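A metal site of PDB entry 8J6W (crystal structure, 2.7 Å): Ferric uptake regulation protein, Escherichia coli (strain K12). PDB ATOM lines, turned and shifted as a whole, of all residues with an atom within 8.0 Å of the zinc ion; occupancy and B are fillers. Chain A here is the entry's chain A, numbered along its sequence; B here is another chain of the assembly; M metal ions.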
ATOM      1  N   ILE A  92       9.950  17.150 -12.969  1.00  0.00           N
ATOM      2  CA  ILE A  92      10.804  17.687 -11.876  1.00  0.00           C
ATOM      3  C   ILE A  92      10.155  18.920 -11.228  1.00  0.00           C
ATOM      4  O   ILE A  92       9.809  19.860 -11.970  1.00  0.00           O
ATOM      5  CB  ILE A  92      12.227  17.999 -12.402  1.00  0.00           C
ATOM      6  CG1 ILE A  92      12.843  16.784 -13.104  1.00  0.00           C
ATOM      7  CG2 ILE A  92      13.127  18.525 -11.300  1.00  0.00           C
ATOM      8  CD1 ILE A  92      12.972  16.938 -14.608  1.00  0.00           C
ATOM      9  N   CYS A  93      10.020  18.908  -9.901  1.00  0.00           N
ATOM     10  CA  CYS A  93       9.471  20.018  -9.151  1.00  0.00           C
ATOM     11  C   CYS A  93      10.561  21.038  -8.861  1.00  0.00           C
ATOM     12  O   CYS A  93      11.573  20.706  -8.232  1.00  0.00           O
ATOM     13  CB  CYS A  93       8.867  19.555  -7.840  1.00  0.00           C
ATOM     14  SG  CYS A  93       8.197  20.941  -6.989  1.00  0.00           S
ATOM     15  N   LEU A  94      10.328  22.284  -9.295  1.00  0.00           N
ATOM     16  CA  LEU A  94      11.319  23.353  -9.220  1.00  0.00           C
ATOM     17  C   LEU A  94      11.444  24.005  -7.840  1.00  0.00           C
ATOM     18  O   LEU A  94      12.420  24.728  -7.617  1.00  0.00           O
ATOM     19  CB  LEU A  94      10.983  24.417 -10.265  1.00  0.00           C
ATOM     20  CG  LEU A  94      11.150  23.955 -11.702  1.00  0.00           C
ATOM     21  CD1 LEU A  94      10.614  24.975 -12.700  1.00  0.00           C
ATOM     22  CD2 LEU A  94      12.627  23.666 -11.961  1.00  0.00           C
ATOM     23  N   ASP A  95      10.519  23.768  -6.917  1.00  0.00           N
ATOM     24  CA  ASP A  95      10.596  24.369  -5.595  1.00  0.00           C
ATOM     25  C   ASP A  95      11.359  23.501  -4.608  1.00  0.00           C
ATOM     26  O   ASP A  95      12.122  24.022  -3.782  1.00  0.00           O
ATOM     27  CB  ASP A  95       9.190  24.618  -5.038  1.00  0.00           C
ATOM     28  CG  ASP A  95       8.433  25.621  -5.852  1.00  0.00           C
ATOM     29  OD1 ASP A  95       8.870  26.787  -5.907  1.00  0.00           O
ATOM     30  OD2 ASP A  95       7.408  25.242  -6.460  1.00  0.00           O
ATOM     31  N   CYS A  96      11.173  22.161  -4.708  1.00  0.00           N
ATOM     32  CA  CYS A  96      11.702  21.183  -3.770  1.00  0.00           C
ATOM     33  C   CYS A  96      12.679  20.186  -4.390  1.00  0.00           C
ATOM     34  O   CYS A  96      13.333  19.451  -3.655  1.00  0.00           O
ATOM     35  CB  CYS A  96      10.554  20.401  -3.115  1.00  0.00           C
ATOM     36  SG  CYS A  96       9.876  19.125  -4.176  1.00  0.00           S
ATOM     37  N   GLY A  97      12.777  20.126  -5.720  1.00  0.00           N
ATOM     38  CA  GLY A  97      13.766  19.296  -6.390  1.00  0.00           C
ATOM     39  C   GLY A  97      13.327  17.888  -6.696  1.00  0.00           C
ATOM     40  O   GLY A  97      14.112  17.145  -7.313  1.00  0.00           O
ATOM     41  N   LYS A  98      12.097  17.526  -6.338  1.00  0.00           N
ATOM     42  CA  LYS A  98      11.629  16.125  -6.515  1.00  0.00           C
ATOM     43  C   LYS A  98      11.614  15.714  -7.982  1.00  0.00           C
ATOM     44  O   LYS A  98      10.988  16.402  -8.783  1.00  0.00           O
ATOM     45  CB  LYS A  98      10.245  15.923  -5.904  1.00  0.00           C
ATOM     46  CG  LYS A  98       9.715  14.498  -5.934  1.00  0.00           C
ATOM     47  CD  LYS A  98      10.004  13.717  -4.678  1.00  0.00           C
ATOM     48  CE  LYS A  98       9.433  12.310  -4.711  1.00  0.00           C
ATOM     49  NZ  LYS A  98       7.952  12.325  -4.755  1.00  0.00           N
ATOM     50  N   VAL A  99      12.278  14.605  -8.308  1.00  0.00           N
ATOM     51  CA  VAL A  99      12.243  14.062  -9.663  1.00  0.00           C
ATOM     52  C   VAL A  99      11.236  12.914  -9.689  1.00  0.00           C
ATOM     53  O   VAL A  99      11.401  11.928  -8.955  1.00  0.00           O
ATOM     54  CB  VAL A  99      13.631  13.563 -10.095  1.00  0.00           C
ATOM     55  CG1 VAL A  99      13.523  12.891 -11.454  1.00  0.00           C
ATOM     56  CG2 VAL A  99      14.638  14.705 -10.093  1.00  0.00           C
ATOM     57  N   ILE A 100      10.205  13.043 -10.512  1.00  0.00           N
ATOM     58  CA  ILE A 100       9.110  12.084 -10.572  1.00  0.00           C
ATOM     59  C   ILE A 100       9.144  11.387 -11.926  1.00  0.00           C
ATOM     60  O   ILE A 100       9.235  12.062 -12.963  1.00  0.00           O
ATOM     61  CB  ILE A 100       7.738  12.759 -10.377  1.00  0.00           C
ATOM     62  CG1 ILE A 100       7.611  13.367  -8.990  1.00  0.00           C
ATOM     63  CG2 ILE A 100       6.619  11.774 -10.648  1.00  0.00           C
ATOM     64  CD1 ILE A 100       7.057  14.768  -9.046  1.00  0.00           C
ATOM     65  N   GLY A 131       8.004  22.357 -13.401  1.00  0.00           N
ATOM     66  CA  GLY A 131       6.881  23.118 -12.895  1.00  0.00           C
ATOM     67  C   GLY A 131       7.036  23.439 -11.423  1.00  0.00           C
ATOM     68  O   GLY A 131       8.048  23.107 -10.793  1.00  0.00           O
ATOM     69  N   HIS A 132       6.011  24.102 -10.879  1.00  0.00           N
ATOM     70  CA  HIS A 132       6.005  24.537  -9.492  1.00  0.00           C
ATOM     71  C   HIS A 132       4.874  23.819  -8.757  1.00  0.00           C
ATOM     72  O   HIS A 132       3.903  23.350  -9.378  1.00  0.00           O
ATOM     73  CB  HIS A 132       5.847  26.072  -9.402  1.00  0.00           C
ATOM     74  CG  HIS A 132       6.967  26.817 -10.051  1.00  0.00           C
ATOM     75  ND1 HIS A 132       7.978  27.402  -9.321  1.00  0.00           N
ATOM     76  CD2 HIS A 132       7.264  27.022 -11.356  1.00  0.00           C
ATOM     77  CE1 HIS A 132       8.851  27.944 -10.152  1.00  0.00           C
ATOM     78  NE2 HIS A 132       8.434  27.729 -11.388  1.00  0.00           N
ATOM     79  N   CYS A 133       4.999  23.727  -7.435  1.00  0.00           N
ATOM     80  CA  CYS A 133       3.945  23.063  -6.678  1.00  0.00           C
ATOM     81  C   CYS A 133       2.668  23.877  -6.780  1.00  0.00           C
ATOM     82  O   CYS A 133       2.663  25.086  -6.548  1.00  0.00           O
ATOM     83  CB  CYS A 133       4.330  22.880  -5.209  1.00  0.00           C
ATOM     84  SG  CYS A 133       4.559  24.389  -4.256  1.00  0.00           S
ATOM     85  N   ALA A 134       1.580  23.209  -7.126  1.00  0.00           N
ATOM     86  CA  ALA A 134       0.321  23.889  -7.373  1.00  0.00           C
ATOM     87  C   ALA A 134      -0.259  24.505  -6.102  1.00  0.00           C
ATOM     88  O   ALA A 134      -0.785  25.631  -6.143  1.00  0.00           O
ATOM     89  CB  ALA A 134      -0.647  22.919  -8.032  1.00  0.00           C
ATOM     90  N   ASP A 137       3.031  24.527  -0.065  1.00  0.00           N
ATOM     91  CA  ASP A 137       4.484  24.512  -0.180  1.00  0.00           C
ATOM     92  C   ASP A 137       4.927  23.066  -0.029  1.00  0.00           C
ATOM     93  O   ASP A 137       4.887  22.507   1.067  1.00  0.00           O
ATOM     94  CB  ASP A 137       5.127  25.419   0.872  1.00  0.00           C
ATOM     95  CG  ASP A 137       6.630  25.548   0.703  1.00  0.00           C
ATOM     96  OD1 ASP A 137       7.113  25.434  -0.442  1.00  0.00           O
ATOM     97  OD2 ASP A 137       7.331  25.805   1.709  1.00  0.00           O
ATOM     98  N   CYS A 138       5.331  22.460  -1.153  1.00  0.00           N
ATOM     99  CA  CYS A 138       5.769  21.073  -1.138  1.00  0.00           C
ATOM    100  C   CYS A 138       7.040  20.861  -0.337  1.00  0.00           C
ATOM    101  O   CYS A 138       7.390  19.718  -0.038  1.00  0.00           O
ATOM    102  CB  CYS A 138       6.008  20.586  -2.554  1.00  0.00           C
ATOM    103  SG  CYS A 138       7.037  21.715  -3.478  1.00  0.00           S
ATOM    104  N   ARG A 139       7.776  21.931  -0.013  1.00  0.00           N
ATOM    105  CA  ARG A 139       8.979  21.772   0.786  1.00  0.00           C
ATOM    106  C   ARG A 139       8.654  21.255   2.172  1.00  0.00           C
ATOM    107  O   ARG A 139       9.574  20.881   2.911  1.00  0.00           O
ATOM    108  CB  ARG A 139       9.732  23.089   0.914  1.00  0.00           C
ATOM    109  CG  ARG A 139      10.363  23.630  -0.349  1.00  0.00           C
ATOM    110  CD  ARG A 139      10.671  25.080  -0.129  1.00  0.00           C
ATOM    111  NE  ARG A 139      10.400  25.847  -1.340  1.00  0.00           N
ATOM    112  CZ  ARG A 139       9.805  27.015  -1.329  1.00  0.00           C
ATOM    113  NH1 ARG A 139       9.437  27.589  -0.186  1.00  0.00           N
ATOM    114  NH2 ARG A 139       9.548  27.631  -2.492  1.00  0.00           N
ATOM    115  N   GLU A 140       7.382  21.250   2.571  1.00  0.00           N
ATOM    116  CA  GLU A 140       6.932  20.646   3.818  1.00  0.00           C
ATOM    117  C   GLU A 140       6.292  19.286   3.612  1.00  0.00           C
ATOM    118  O   GLU A 140       6.759  18.291   4.178  1.00  0.00           O
ATOM    119  CB  GLU A 140       5.956  21.588   4.515  1.00  0.00           C
ATOM    120  CG  GLU A 140       6.442  23.010   4.501  1.00  0.00           C
ATOM    121  CD  GLU A 140       7.719  23.146   5.306  1.00  0.00           C
ATOM    122  OE1 GLU A 140       7.739  22.707   6.479  1.00  0.00           O
ATOM    123  OE2 GLU A 140       8.698  23.719   4.791  1.00  0.00           O
ATOM    124  N   ASP A 141       5.245  19.222   2.790  1.00  0.00           N
ATOM    125  CA  ASP A 141       4.476  18.002   2.559  1.00  0.00           C
ATOM    126  C   ASP A 141       5.268  17.039   1.689  1.00  0.00           C
ATOM    127  O   ASP A 141       5.244  17.132   0.465  1.00  0.00           O
ATOM    128  CB  ASP A 141       3.142  18.349   1.929  1.00  0.00           C
ATOM    129  CG  ASP A 141       2.244  17.138   1.801  1.00  0.00           C
ATOM    130  OD1 ASP A 141       2.544  16.125   2.474  1.00  0.00           O
ATOM    131  OD2 ASP A 141       1.240  17.214   1.036  1.00  0.00           O
ATOM    132  N   ALA A 144       3.480  15.624  -1.233  1.00  0.00           N
ATOM    133  CA  ALA A 144       2.939  16.585  -2.192  1.00  0.00           C
ATOM    134  C   ALA A 144       2.892  16.026  -3.614  1.00  0.00           C
ATOM    135  O   ALA A 144       1.972  16.358  -4.360  1.00  0.00           O
ATOM    136  CB  ALA A 144       3.745  17.881  -2.182  1.00  0.00           C
ATOM    137  N   HIS A 145       3.847  15.180  -3.984  1.00  0.00           N
ATOM    138  CA  HIS A 145       3.977  14.761  -5.375  1.00  0.00           C
ATOM    139  C   HIS A 145       3.700  13.274  -5.584  1.00  0.00           C
ATOM    140  O   HIS A 145       4.141  12.719  -6.599  1.00  0.00           O
ATOM    141  CB  HIS A 145       5.363  15.125  -5.908  1.00  0.00           C
ATOM    142  CG  HIS A 145       5.716  16.563  -5.778  1.00  0.00           C
ATOM    143  ND1 HIS A 145       4.854  17.580  -6.142  1.00  0.00           N
ATOM    144  CD2 HIS A 145       6.846  17.181  -5.341  1.00  0.00           C
ATOM    145  CE1 HIS A 145       5.424  18.745  -5.928  1.00  0.00           C
ATOM    146  NE2 HIS A 145       6.636  18.542  -5.434  1.00  0.00           N
ATOM    147  N   HIS B 118       0.570  15.035 -10.084  1.00  0.00           N
ATOM    148  CA  HIS B 118       1.572  14.915  -9.031  1.00  0.00           C
ATOM    149  C   HIS B 118       1.763  16.203  -8.258  1.00  0.00           C
ATOM    150  O   HIS B 118       2.859  16.423  -7.720  1.00  0.00           O
ATOM    151  CB  HIS B 118       2.903  14.459  -9.611  1.00  0.00           C
ATOM    152  CG  HIS B 118       2.896  13.075 -10.182  1.00  0.00           C
ATOM    153  ND1 HIS B 118       2.366  12.776 -11.406  1.00  0.00           N
ATOM    154  CD2 HIS B 118       3.385  11.912  -9.689  1.00  0.00           C
ATOM    155  CE1 HIS B 118       2.534  11.495 -11.664  1.00  0.00           C
ATOM    156  NE2 HIS B 118       3.138  10.945 -10.631  1.00  0.00           N
ATOM    157  N   GLY B 119       0.749  17.057  -8.194  1.00  0.00           N
ATOM    158  CA  GLY B 119       0.832  18.290  -7.438  1.00  0.00           C
ATOM    159  C   GLY B 119       1.564  19.443  -8.093  1.00  0.00           C
ATOM    160  O   GLY B 119       1.889  20.421  -7.400  1.00  0.00           O
ATOM    161  N   ILE B 120       1.829  19.388  -9.400  1.00  0.00           N
ATOM    162  CA  ILE B 120       2.702  20.335 -10.069  1.00  0.00           C
ATOM    163  C   ILE B 120       1.915  21.082 -11.127  1.00  0.00           C
ATOM    164  O   ILE B 120       1.117  20.483 -11.849  1.00  0.00           O
ATOM    165  CB  ILE B 120       3.935  19.651 -10.712  1.00  0.00           C
ATOM    166  CG1 ILE B 120       4.956  19.278  -9.627  1.00  0.00           C
ATOM    167  CG2 ILE B 120       4.566  20.517 -11.802  1.00  0.00           C
ATOM    168  CD1 ILE B 120       5.757  18.066  -9.949  1.00  0.00           C
HETATM  169 ZN    ZN M   1       7.903  20.139  -4.892  1.00  0.00          ZN
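The backbone carbonyl oxygen (O) of His 118 of chain B lies within hydrogen-bond range of a ring nitrogen (ND1) of His 145, 2.8 Å away.
The side-chain sulfur (SG) of Cys 93 sits close to the backbone NH (N) of Asp 95, at 3.7 Å.
N of Cys 93 is in hydrogen-bond range of O of Lys 98, 2.9 Å away.
N of Cys 138 lies within hydrogen-bond range of SG of Cys 133.
The side-chain sulfur (SG) of Cys 96 sits close to the backbone NH (N) of Lys 98.
Four residues have an atom within 4 Å of the zinc ion: Cys 93, Cys 96, Cys 138 and His 145.
The zinc ion is bound by a ring nitrogen (NE2) of His 145, the side-chain sulfur of Cys 93, the side-chain sulfur of Cys 138 and the side-chain sulfur of Cys 96.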
